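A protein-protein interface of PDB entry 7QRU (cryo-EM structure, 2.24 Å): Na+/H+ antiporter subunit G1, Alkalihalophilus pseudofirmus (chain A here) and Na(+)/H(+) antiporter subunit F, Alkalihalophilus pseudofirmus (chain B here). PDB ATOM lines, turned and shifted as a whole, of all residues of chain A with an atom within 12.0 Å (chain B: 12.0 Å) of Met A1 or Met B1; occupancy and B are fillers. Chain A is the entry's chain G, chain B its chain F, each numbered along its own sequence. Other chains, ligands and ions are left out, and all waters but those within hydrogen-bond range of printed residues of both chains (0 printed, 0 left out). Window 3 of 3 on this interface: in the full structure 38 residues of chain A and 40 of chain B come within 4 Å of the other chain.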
ATOM      1  N   MET A   1       6.825 -17.201  -6.918  1.00  0.00           N
ATOM      2  CA  MET A   1       6.263 -18.131  -7.935  1.00  0.00           C
ATOM      3  C   MET A   1       5.651 -19.397  -7.306  1.00  0.00           C
ATOM      4  O   MET A   1       6.363 -20.165  -6.668  1.00  0.00           O
ATOM      5  CB  MET A   1       7.346 -18.523  -8.950  1.00  0.00           C
ATOM      6  CG  MET A   1       6.823 -18.453 -10.381  1.00  0.00           C
ATOM      7  SD  MET A   1       7.928 -18.965 -11.742  1.00  0.00           S
ATOM      8  CE  MET A   1       6.929 -18.271 -13.040  1.00  0.00           C
ATOM      9  N   THR A   2       4.343 -19.637  -7.539  1.00  0.00           N
ATOM     10  CA  THR A   2       3.575 -20.746  -6.954  1.00  0.00           C
ATOM     11  C   THR A   2       3.904 -22.067  -7.628  1.00  0.00           C
ATOM     12  O   THR A   2       4.400 -22.029  -8.742  1.00  0.00           O
ATOM     13  CB  THR A   2       2.077 -20.442  -7.042  1.00  0.00           C
ATOM     14  OG1 THR A   2       1.599 -20.139  -8.356  1.00  0.00           O
ATOM     15  CG2 THR A   2       1.752 -19.227  -6.197  1.00  0.00           C
ATOM     16  N   ALA A   3       3.669 -23.212  -6.983  1.00  0.00           N
ATOM     17  CA  ALA A   3       4.022 -24.467  -7.639  1.00  0.00           C
ATOM     18  C   ALA A   3       3.260 -24.659  -8.955  1.00  0.00           C
ATOM     19  O   ALA A   3       3.793 -25.317  -9.845  1.00  0.00           O
ATOM     20  CB  ALA A   3       3.747 -25.653  -6.777  1.00  0.00           C
ATOM     21  N   VAL A   4       2.017 -24.140  -9.090  1.00  0.00           N
ATOM     22  CA  VAL A   4       1.368 -24.219 -10.387  1.00  0.00           C
ATOM     23  C   VAL A   4       2.161 -23.368 -11.385  1.00  0.00           C
ATOM     24  O   VAL A   4       2.448 -23.855 -12.478  1.00  0.00           O
ATOM     25  CB  VAL A   4      -0.116 -23.832 -10.430  1.00  0.00           C
ATOM     26  CG1 VAL A   4      -0.931 -24.961  -9.856  1.00  0.00           C
ATOM     27  CG2 VAL A   4      -0.369 -22.499  -9.749  1.00  0.00           C
ATOM     28  N   GLU A   5       2.490 -22.129 -11.048  1.00  0.00           N
ATOM     29  CA  GLU A   5       3.250 -21.306 -11.972  1.00  0.00           C
ATOM     30  C   GLU A   5       4.582 -21.963 -12.368  1.00  0.00           C
ATOM     31  O   GLU A   5       5.071 -21.714 -13.458  1.00  0.00           O
ATOM     32  CB  GLU A   5       3.507 -19.906 -11.422  1.00  0.00           C
ATOM     33  CG  GLU A   5       2.301 -19.064 -11.547  1.00  0.00           C
ATOM     34  CD  GLU A   5       2.379 -17.686 -10.904  1.00  0.00           C
ATOM     35  OE1 GLU A   5       3.362 -17.441 -10.174  1.00  0.00           O
ATOM     36  OE2 GLU A   5       1.443 -16.843 -11.143  1.00  0.00           O
ATOM     37  N   ILE A   6       5.155 -22.827 -11.549  1.00  0.00           N
ATOM     38  CA  ILE A   6       6.422 -23.410 -11.921  1.00  0.00           C
ATOM     39  C   ILE A   6       6.188 -24.497 -12.960  1.00  0.00           C
ATOM     40  O   ILE A   6       6.943 -24.632 -13.898  1.00  0.00           O
ATOM     41  CB  ILE A   6       7.167 -23.941 -10.681  1.00  0.00           C
ATOM     42  CG1 ILE A   6       7.674 -22.785  -9.825  1.00  0.00           C
ATOM     43  CG2 ILE A   6       8.295 -24.832 -11.088  1.00  0.00           C
ATOM     44  CD1 ILE A   6       8.103 -23.271  -8.486  1.00  0.00           C
ATOM     45  N   ILE A   7       5.175 -25.312 -12.774  1.00  0.00           N
ATOM     46  CA  ILE A   7       4.884 -26.367 -13.729  1.00  0.00           C
ATOM     47  C   ILE A   7       4.529 -25.740 -15.091  1.00  0.00           C
ATOM     48  O   ILE A   7       4.919 -26.206 -16.132  1.00  0.00           O
ATOM     49  CB  ILE A   7       3.734 -27.199 -13.158  1.00  0.00           C
ATOM     50  CG1 ILE A   7       4.228 -28.002 -11.970  1.00  0.00           C
ATOM     51  CG2 ILE A   7       3.140 -28.091 -14.218  1.00  0.00           C
ATOM     52  CD1 ILE A   7       3.106 -28.372 -11.026  1.00  0.00           C
ATOM     53  N   ILE A   8       3.691 -24.713 -15.081  1.00  0.00           N
ATOM     54  CA  ILE A   8       3.294 -24.054 -16.294  1.00  0.00           C
ATOM     55  C   ILE A   8       4.507 -23.407 -16.919  1.00  0.00           C
ATOM     56  O   ILE A   8       4.603 -23.467 -18.126  1.00  0.00           O
ATOM     57  CB  ILE A   8       2.204 -23.004 -15.997  1.00  0.00           C
ATOM     58  CG1 ILE A   8       0.938 -23.731 -15.564  1.00  0.00           C
ATOM     59  CG2 ILE A   8       1.966 -22.128 -17.206  1.00  0.00           C
ATOM     60  CD1 ILE A   8      -0.026 -22.751 -15.169  1.00  0.00           C
ATOM     61  N   SER A   9       5.356 -22.741 -16.119  1.00  0.00           N
ATOM     62  CA  SER A   9       6.641 -22.221 -16.594  1.00  0.00           C
ATOM     63  C   SER A   9       7.475 -23.265 -17.327  1.00  0.00           C
ATOM     64  O   SER A   9       7.998 -22.968 -18.389  1.00  0.00           O
ATOM     65  CB  SER A   9       7.371 -21.609 -15.516  1.00  0.00           C
ATOM     66  OG  SER A   9       6.575 -20.463 -15.232  1.00  0.00           O
ATOM     67  N   ILE A  10       7.542 -24.486 -16.834  1.00  0.00           N
ATOM     68  CA  ILE A  10       8.453 -25.410 -17.471  1.00  0.00           C
ATOM     69  C   ILE A  10       7.955 -25.671 -18.886  1.00  0.00           C
ATOM     70  O   ILE A  10       8.683 -25.595 -19.820  1.00  0.00           O
ATOM     71  CB  ILE A  10       8.594 -26.700 -16.630  1.00  0.00           C
ATOM     72  CG1 ILE A  10       9.482 -26.489 -15.421  1.00  0.00           C
ATOM     73  CG2 ILE A  10       9.138 -27.811 -17.425  1.00  0.00           C
ATOM     74  CD1 ILE A  10       9.030 -27.382 -14.285  1.00  0.00           C
ATOM     75  N   PHE A  11       6.701 -26.049 -19.002  1.00  0.00           N
ATOM     76  CA  PHE A  11       6.015 -26.230 -20.252  1.00  0.00           C
ATOM     77  C   PHE A  11       6.155 -25.016 -21.171  1.00  0.00           C
ATOM     78  O   PHE A  11       6.430 -25.248 -22.324  1.00  0.00           O
ATOM     79  CB  PHE A  11       4.569 -26.546 -19.901  1.00  0.00           C
ATOM     80  CG  PHE A  11       4.408 -27.978 -19.523  1.00  0.00           C
ATOM     81  CD1 PHE A  11       4.833 -28.954 -20.404  1.00  0.00           C
ATOM     82  CD2 PHE A  11       3.915 -28.350 -18.286  1.00  0.00           C
ATOM     83  CE1 PHE A  11       4.750 -30.287 -20.046  1.00  0.00           C
ATOM     84  CE2 PHE A  11       3.845 -29.681 -17.928  1.00  0.00           C
ATOM     85  CZ  PHE A  11       4.258 -30.642 -18.809  1.00  0.00           C
ATOM     86  N   VAL A  12       5.984 -23.765 -20.723  1.00  0.00           N
ATOM     87  CA  VAL A  12       6.162 -22.703 -21.675  1.00  0.00           C
ATOM     88  C   VAL A  12       7.641 -22.512 -22.037  1.00  0.00           C
ATOM     89  O   VAL A  12       7.882 -22.192 -23.208  1.00  0.00           O
ATOM     90  CB  VAL A  12       5.572 -21.337 -21.297  1.00  0.00           C
ATOM     91  CG1 VAL A  12       4.184 -21.520 -20.914  1.00  0.00           C
ATOM     92  CG2 VAL A  12       6.280 -20.739 -20.148  1.00  0.00           C
ATOM     93  N   LEU A  13       8.591 -22.740 -21.125  1.00  0.00           N
ATOM     94  CA  LEU A  13       9.982 -22.559 -21.496  1.00  0.00           C
ATOM     95  C   LEU A  13      10.421 -23.682 -22.411  1.00  0.00           C
ATOM     96  O   LEU A  13      11.006 -23.358 -23.408  1.00  0.00           O
ATOM     97  CB  LEU A  13      10.920 -22.545 -20.320  1.00  0.00           C
ATOM     98  CG  LEU A  13      10.738 -21.295 -19.497  1.00  0.00           C
ATOM     99  CD1 LEU A  13      11.361 -21.537 -18.168  1.00  0.00           C
ATOM    100  CD2 LEU A  13      11.344 -20.112 -20.184  1.00  0.00           C
ATOM    101  N   ILE A  14       9.975 -24.915 -22.229  1.00  0.00           N
ATOM    102  CA  ILE A  14      10.273 -25.950 -23.204  1.00  0.00           C
ATOM    103  C   ILE A  14       9.627 -25.607 -24.552  1.00  0.00           C
ATOM    104  O   ILE A  14      10.204 -25.820 -25.607  1.00  0.00           O
ATOM    105  CB  ILE A  14       9.791 -27.309 -22.671  1.00  0.00           C
ATOM    106  CG1 ILE A  14      10.646 -27.717 -21.475  1.00  0.00           C
ATOM    107  CG2 ILE A  14       9.766 -28.376 -23.739  1.00  0.00           C
ATOM    108  CD1 ILE A  14      10.005 -28.855 -20.699  1.00  0.00           C
ATOM    109  N   ALA A  53       0.615 -25.977 -21.462  1.00  0.00           N
ATOM    110  CA  ALA A  53       0.801 -24.933 -20.469  1.00  0.00           C
ATOM    111  C   ALA A  53      -0.465 -24.099 -20.438  1.00  0.00           C
ATOM    112  O   ALA A  53      -1.032 -23.851 -19.405  1.00  0.00           O
ATOM    113  CB  ALA A  53       2.040 -24.052 -20.816  1.00  0.00           C
ATOM    114  N   PHE A  57      -2.879 -23.854 -17.400  1.00  0.00           N
ATOM    115  CA  PHE A  57      -3.047 -22.541 -16.803  1.00  0.00           C
ATOM    116  C   PHE A  57      -4.512 -22.225 -16.555  1.00  0.00           C
ATOM    117  O   PHE A  57      -4.835 -21.740 -15.510  1.00  0.00           O
ATOM    118  CB  PHE A  57      -2.451 -21.522 -17.753  1.00  0.00           C
ATOM    119  CG  PHE A  57      -2.647 -20.133 -17.305  1.00  0.00           C
ATOM    120  CD1 PHE A  57      -1.873 -19.632 -16.288  1.00  0.00           C
ATOM    121  CD2 PHE A  57      -3.636 -19.335 -17.894  1.00  0.00           C
ATOM    122  CE1 PHE A  57      -2.063 -18.332 -15.846  1.00  0.00           C
ATOM    123  CE2 PHE A  57      -3.858 -18.045 -17.409  1.00  0.00           C
ATOM    124  CZ  PHE A  57      -3.033 -17.534 -16.414  1.00  0.00           C
ATOM    125  N   VAL A  61      -5.461 -22.568 -12.576  1.00  0.00           N
ATOM    126  CA  VAL A  61      -5.464 -21.218 -12.052  1.00  0.00           C
ATOM    127  C   VAL A  61      -6.837 -20.563 -12.183  1.00  0.00           C
ATOM    128  O   VAL A  61      -7.127 -19.697 -11.370  1.00  0.00           O
ATOM    129  CB  VAL A  61      -4.368 -20.371 -12.732  1.00  0.00           C
ATOM    130  CG1 VAL A  61      -4.265 -18.974 -12.218  1.00  0.00           C
ATOM    131  CG2 VAL A  61      -3.018 -21.057 -12.638  1.00  0.00           C
ATOM    132  N   MET B   1       6.757 -12.143 -12.257  1.00  0.00           N
ATOM    133  CA  MET B   1       7.861 -13.161 -12.489  1.00  0.00           C
ATOM    134  C   MET B   1       7.455 -14.305 -13.432  1.00  0.00           C
ATOM    135  O   MET B   1       8.178 -14.633 -14.358  1.00  0.00           O
ATOM    136  CB  MET B   1       8.343 -13.835 -11.213  1.00  0.00           C
ATOM    137  CG  MET B   1       8.948 -15.241 -11.455  1.00  0.00           C
ATOM    138  SD  MET B   1      10.615 -15.238 -12.116  1.00  0.00           S
ATOM    139  CE  MET B   1      11.340 -16.590 -11.181  1.00  0.00           C
ATOM    140  N   PHE B   2       6.297 -14.929 -13.164  1.00  0.00           N
ATOM    141  CA  PHE B   2       5.565 -15.684 -14.154  1.00  0.00           C
ATOM    142  C   PHE B   2       5.240 -14.809 -15.385  1.00  0.00           C
ATOM    143  O   PHE B   2       5.538 -15.205 -16.478  1.00  0.00           O
ATOM    144  CB  PHE B   2       4.357 -16.300 -13.490  1.00  0.00           C
ATOM    145  CG  PHE B   2       3.577 -17.157 -14.430  1.00  0.00           C
ATOM    146  CD1 PHE B   2       4.150 -18.288 -14.957  1.00  0.00           C
ATOM    147  CD2 PHE B   2       2.381 -16.688 -14.958  1.00  0.00           C
ATOM    148  CE1 PHE B   2       3.434 -19.034 -15.873  1.00  0.00           C
ATOM    149  CE2 PHE B   2       1.680 -17.433 -15.883  1.00  0.00           C
ATOM    150  CZ  PHE B   2       2.215 -18.596 -16.353  1.00  0.00           C
ATOM    151  N   GLN B   3       4.821 -13.585 -15.242  1.00  0.00           N
ATOM    152  CA  GLN B   3       4.597 -12.752 -16.396  1.00  0.00           C
ATOM    153  C   GLN B   3       5.914 -12.393 -17.080  1.00  0.00           C
ATOM    154  O   GLN B   3       5.911 -12.121 -18.274  1.00  0.00           O
ATOM    155  CB  GLN B   3       3.868 -11.459 -16.011  1.00  0.00           C
ATOM    156  CG  GLN B   3       2.546 -11.695 -15.324  1.00  0.00           C
ATOM    157  CD  GLN B   3       1.432 -11.814 -16.317  1.00  0.00           C
ATOM    158  OE1 GLN B   3       1.170 -10.898 -17.095  1.00  0.00           O
ATOM    159  NE2 GLN B   3       0.746 -12.947 -16.272  1.00  0.00           N
ATOM    160  N   SER B   4       7.019 -12.327 -16.360  1.00  0.00           N
ATOM    161  CA  SER B   4       8.334 -12.095 -16.961  1.00  0.00           C
ATOM    162  C   SER B   4       8.775 -13.259 -17.851  1.00  0.00           C
ATOM    163  O   SER B   4       9.197 -13.083 -18.950  1.00  0.00           O
ATOM    164  CB  SER B   4       9.342 -11.885 -15.889  1.00  0.00           C
ATOM    165  OG  SER B   4       9.211 -10.546 -15.439  1.00  0.00           O
ATOM    166  N   ILE B   5       8.643 -14.464 -17.373  1.00  0.00           N
ATOM    167  CA  ILE B   5       8.839 -15.592 -18.202  1.00  0.00           C
ATOM    168  C   ILE B   5       7.909 -15.572 -19.422  1.00  0.00           C
ATOM    169  O   ILE B   5       8.355 -15.983 -20.520  1.00  0.00           O
ATOM    170  CB  ILE B   5       8.624 -16.890 -17.390  1.00  0.00           C
ATOM    171  CG1 ILE B   5       9.752 -17.052 -16.386  1.00  0.00           C
ATOM    172  CG2 ILE B   5       8.542 -18.153 -18.314  1.00  0.00           C
ATOM    173  CD1 ILE B   5       9.490 -18.068 -15.365  1.00  0.00           C
ATOM    174  N   LEU B   6       6.605 -15.305 -19.273  1.00  0.00           N
ATOM    175  CA  LEU B   6       5.811 -15.283 -20.498  1.00  0.00           C
ATOM    176  C   LEU B   6       6.365 -14.243 -21.448  1.00  0.00           C
ATOM    177  O   LEU B   6       6.447 -14.556 -22.593  1.00  0.00           O
ATOM    178  CB  LEU B   6       4.347 -15.001 -20.249  1.00  0.00           C
ATOM    179  CG  LEU B   6       3.697 -16.004 -19.313  1.00  0.00           C
ATOM    180  CD1 LEU B   6       2.357 -15.506 -18.949  1.00  0.00           C
ATOM    181  CD2 LEU B   6       3.583 -17.333 -19.957  1.00  0.00           C
ATOM    182  N   MET B   7       6.827 -13.070 -21.012  1.00  0.00           N
ATOM    183  CA  MET B   7       7.413 -12.134 -21.958  1.00  0.00           C
ATOM    184  C   MET B   7       8.668 -12.659 -22.636  1.00  0.00           C
ATOM    185  O   MET B   7       8.807 -12.522 -23.831  1.00  0.00           O
ATOM    186  CB  MET B   7       7.768 -10.808 -21.312  1.00  0.00           C
ATOM    187  CG  MET B   7       6.516  -9.951 -21.115  1.00  0.00           C
ATOM    188  SD  MET B   7       5.907  -9.028 -22.608  1.00  0.00           S
ATOM    189  CE  MET B   7       7.422  -8.997 -23.545  1.00  0.00           C
ATOM    190  N   ILE B   8       9.573 -13.278 -21.898  1.00  0.00           N
ATOM    191  CA  ILE B   8      10.731 -13.872 -22.508  1.00  0.00           C
ATOM    192  C   ILE B   8      10.319 -14.900 -23.557  1.00  0.00           C
ATOM    193  O   ILE B   8      10.759 -14.862 -24.692  1.00  0.00           O
ATOM    194  CB  ILE B   8      11.614 -14.479 -21.423  1.00  0.00           C
ATOM    195  CG1 ILE B   8      12.318 -13.394 -20.648  1.00  0.00           C
ATOM    196  CG2 ILE B   8      12.625 -15.447 -21.980  1.00  0.00           C
ATOM    197  CD1 ILE B   8      12.856 -13.954 -19.368  1.00  0.00           C
ATOM    198  N   VAL B   9       9.409 -15.779 -23.265  1.00  0.00           N
ATOM    199  CA  VAL B   9       9.004 -16.725 -24.294  1.00  0.00           C
ATOM    200  C   VAL B   9       8.336 -16.059 -25.483  1.00  0.00           C
ATOM    201  O   VAL B   9       8.593 -16.501 -26.595  1.00  0.00           O
ATOM    202  CB  VAL B   9       8.123 -17.810 -23.710  1.00  0.00           C
ATOM    203  CG1 VAL B   9       7.682 -18.782 -24.757  1.00  0.00           C
ATOM    204  CG2 VAL B   9       8.973 -18.497 -22.669  1.00  0.00           C
ATOM    205  N   LEU B  10       7.593 -14.962 -25.310  1.00  0.00           N
ATOM    206  CA  LEU B  10       7.053 -14.331 -26.506  1.00  0.00           C
ATOM    207  C   LEU B  10       8.164 -13.733 -27.338  1.00  0.00           C
ATOM    208  O   LEU B  10       8.027 -13.692 -28.535  1.00  0.00           O
ATOM    209  CB  LEU B  10       6.053 -13.262 -26.096  1.00  0.00           C
ATOM    210  CG  LEU B  10       4.692 -13.783 -25.645  1.00  0.00           C
ATOM    211  CD1 LEU B  10       3.922 -12.635 -25.090  1.00  0.00           C
ATOM    212  CD2 LEU B  10       3.956 -14.415 -26.791  1.00  0.00           C
ATOM    213  N   VAL B  50       0.547 -18.327 -25.729  1.00  0.00           N
ATOM    214  CA  VAL B  50       1.191 -17.606 -24.661  1.00  0.00           C
ATOM    215  C   VAL B  50       0.507 -16.250 -24.542  1.00  0.00           C
ATOM    216  O   VAL B  50       0.440 -15.730 -23.473  1.00  0.00           O
ATOM    217  CB  VAL B  50       2.703 -17.433 -24.924  1.00  0.00           C
ATOM    218  CG1 VAL B  50       3.338 -16.581 -23.874  1.00  0.00           C
ATOM    219  CG2 VAL B  50       3.417 -18.723 -25.051  1.00  0.00           C
ATOM    220  N   MET B  53      -2.289 -16.625 -22.042  1.00  0.00           N
ATOM    221  CA  MET B  53      -1.891 -16.650 -20.613  1.00  0.00           C
ATOM    222  C   MET B  53      -1.512 -15.275 -20.102  1.00  0.00           C
ATOM    223  O   MET B  53      -1.767 -14.941 -18.966  1.00  0.00           O
ATOM    224  CB  MET B  53      -0.700 -17.567 -20.342  1.00  0.00           C
ATOM    225  CG  MET B  53      -0.965 -19.017 -20.775  1.00  0.00           C
ATOM    226  SD  MET B  53       0.290 -20.186 -20.229  1.00  0.00           S
ATOM    227  CE  MET B  53       1.144 -20.450 -21.781  1.00  0.00           C
ATOM    228  N   LEU B  54      -0.871 -14.468 -20.914  1.00  0.00           N
ATOM    229  CA  LEU B  54      -0.491 -13.126 -20.507  1.00  0.00           C
ATOM    230  C   LEU B  54      -1.666 -12.149 -20.390  1.00  0.00           C
ATOM    231  O   LEU B  54      -1.680 -11.350 -19.477  1.00  0.00           O
ATOM    232  CB  LEU B  54       0.506 -12.664 -21.568  1.00  0.00           C
ATOM    233  CG  LEU B  54       1.327 -11.451 -21.248  1.00  0.00           C
ATOM    234  CD1 LEU B  54       2.302 -11.764 -20.159  1.00  0.00           C
ATOM    235  CD2 LEU B  54       2.021 -11.042 -22.503  1.00  0.00           C
ATOM    236  N   GLU B  56      -4.524 -13.265 -19.976  1.00  0.00           N
ATOM    237  CA  GLU B  56      -5.433 -14.118 -19.190  1.00  0.00           C
ATOM    238  C   GLU B  56      -6.863 -14.208 -19.786  1.00  0.00           C
ATOM    239  O   GLU B  56      -7.867 -13.982 -19.102  1.00  0.00           O
ATOM    240  CB  GLU B  56      -5.580 -13.610 -17.766  1.00  0.00           C
ATOM    241  CG  GLU B  56      -4.447 -13.838 -16.831  1.00  0.00           C
ATOM    242  CD  GLU B  56      -3.350 -12.787 -16.926  1.00  0.00           C
ATOM    243  OE1 GLU B  56      -3.633 -11.679 -17.461  1.00  0.00           O
ATOM    244  OE2 GLU B  56      -2.183 -13.090 -16.502  1.00  0.00           O
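The side-chain amide nitrogen (NE2) of Gln B3 sits at hydrogen-bond distance from the side-chain carboxylate (OE2) of Glu B56 (2.9 Å). The side-chain hydroxyl of Thr A2 lies close to the backbone NH of Glu A5. O of Glu A5 is in hydrogen-bond range of OG of Ser A9, 2.6 Å away.
Met B1 touches Met A1. Met A1 touches Phe B2 (CE to CA, 3.1 Å). CB of Phe B2 touches CD of Glu A5, 3.5 Å away. Ile A8 touches Met B53. Ser A9 touches Ile B5. O of Val A12 touches CG1 of Val B9, 3.8 Å away. CG2 of Val B9 touches CD2 of Leu A13, 3.8 Å away. CB of Ala A53 touches CE of Met B53 (3.8 Å). Phe B2 touches Phe A57 (CE2 to CE1, 3.8 Å). CZ of Phe A57 touches O of Met B53, at 3.9 Å.
Met A1 touches three residues of chain B. No residue of chain B comes within 4 Å of Thr A2. No residue of chain B comes within 4 Å of Ala A3. Of chain B, only Phe B2 (3.5 Å) comes within 4 Å of Glu A5. Of the printed residues of chain B, Ile A8 touches Phe B2 (3.6 Å) and Met B53 (3.96 Å). Ser A9 touches just these residues of chain B: Phe B2 and Ile B5. Phe A11 touches none of the printed residues of chain B. Of the printed residues of chain B, Val A12 touches Ile B5, Val B9 and Met B53. Of the printed residues of chain B, Leu A13 touches Ile B5 (3.9 Å) and Val B9 (3.8 Å). Met B1 touches one residue of chain A. Of chain A, only Met A1 (3.1 Å), Glu A5 (3.5 Å), Ile A8 (3.6 Å), Ser A9 (3.3 Å) and Phe A57 (3.8 Å) come within 4 Å of Phe B2. Ile B5 touches just these residues of chain A: Met A1 (3.5 Å), Ser A9 (3.8 Å), Val A12 (3.9 Å) and Leu A13 (3.9 Å). Printed residues of chain A within 4 Å of Val B9: Val A12 and Leu A13. Of the printed residues of chain A, Glu B56 touches Phe A57.
Of the 17 printed residues of chain A, 8 touch a printed residue of chain B. Printed residues of chain A that touch a printed residue of chain B: Met A1, Glu A5, Ile A8, Ser A9, Val A12, Leu A13, Ala A53 and Phe A57. Of the 14 printed residues of chain B, 6 touch a printed residue of chain A. Hydrophobic or aromatic side chains of chain B within 4 Å of the printed part of chain A: Met B1, Phe B2, Ile B5, Val B9 and Met B53. Among the printed residues, 17 pairs touch across the chains. Among the printed residues, no Asp or Glu carboxylate lies within 4 Å of a Lys or Arg side-chain nitrogen of the other chain.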
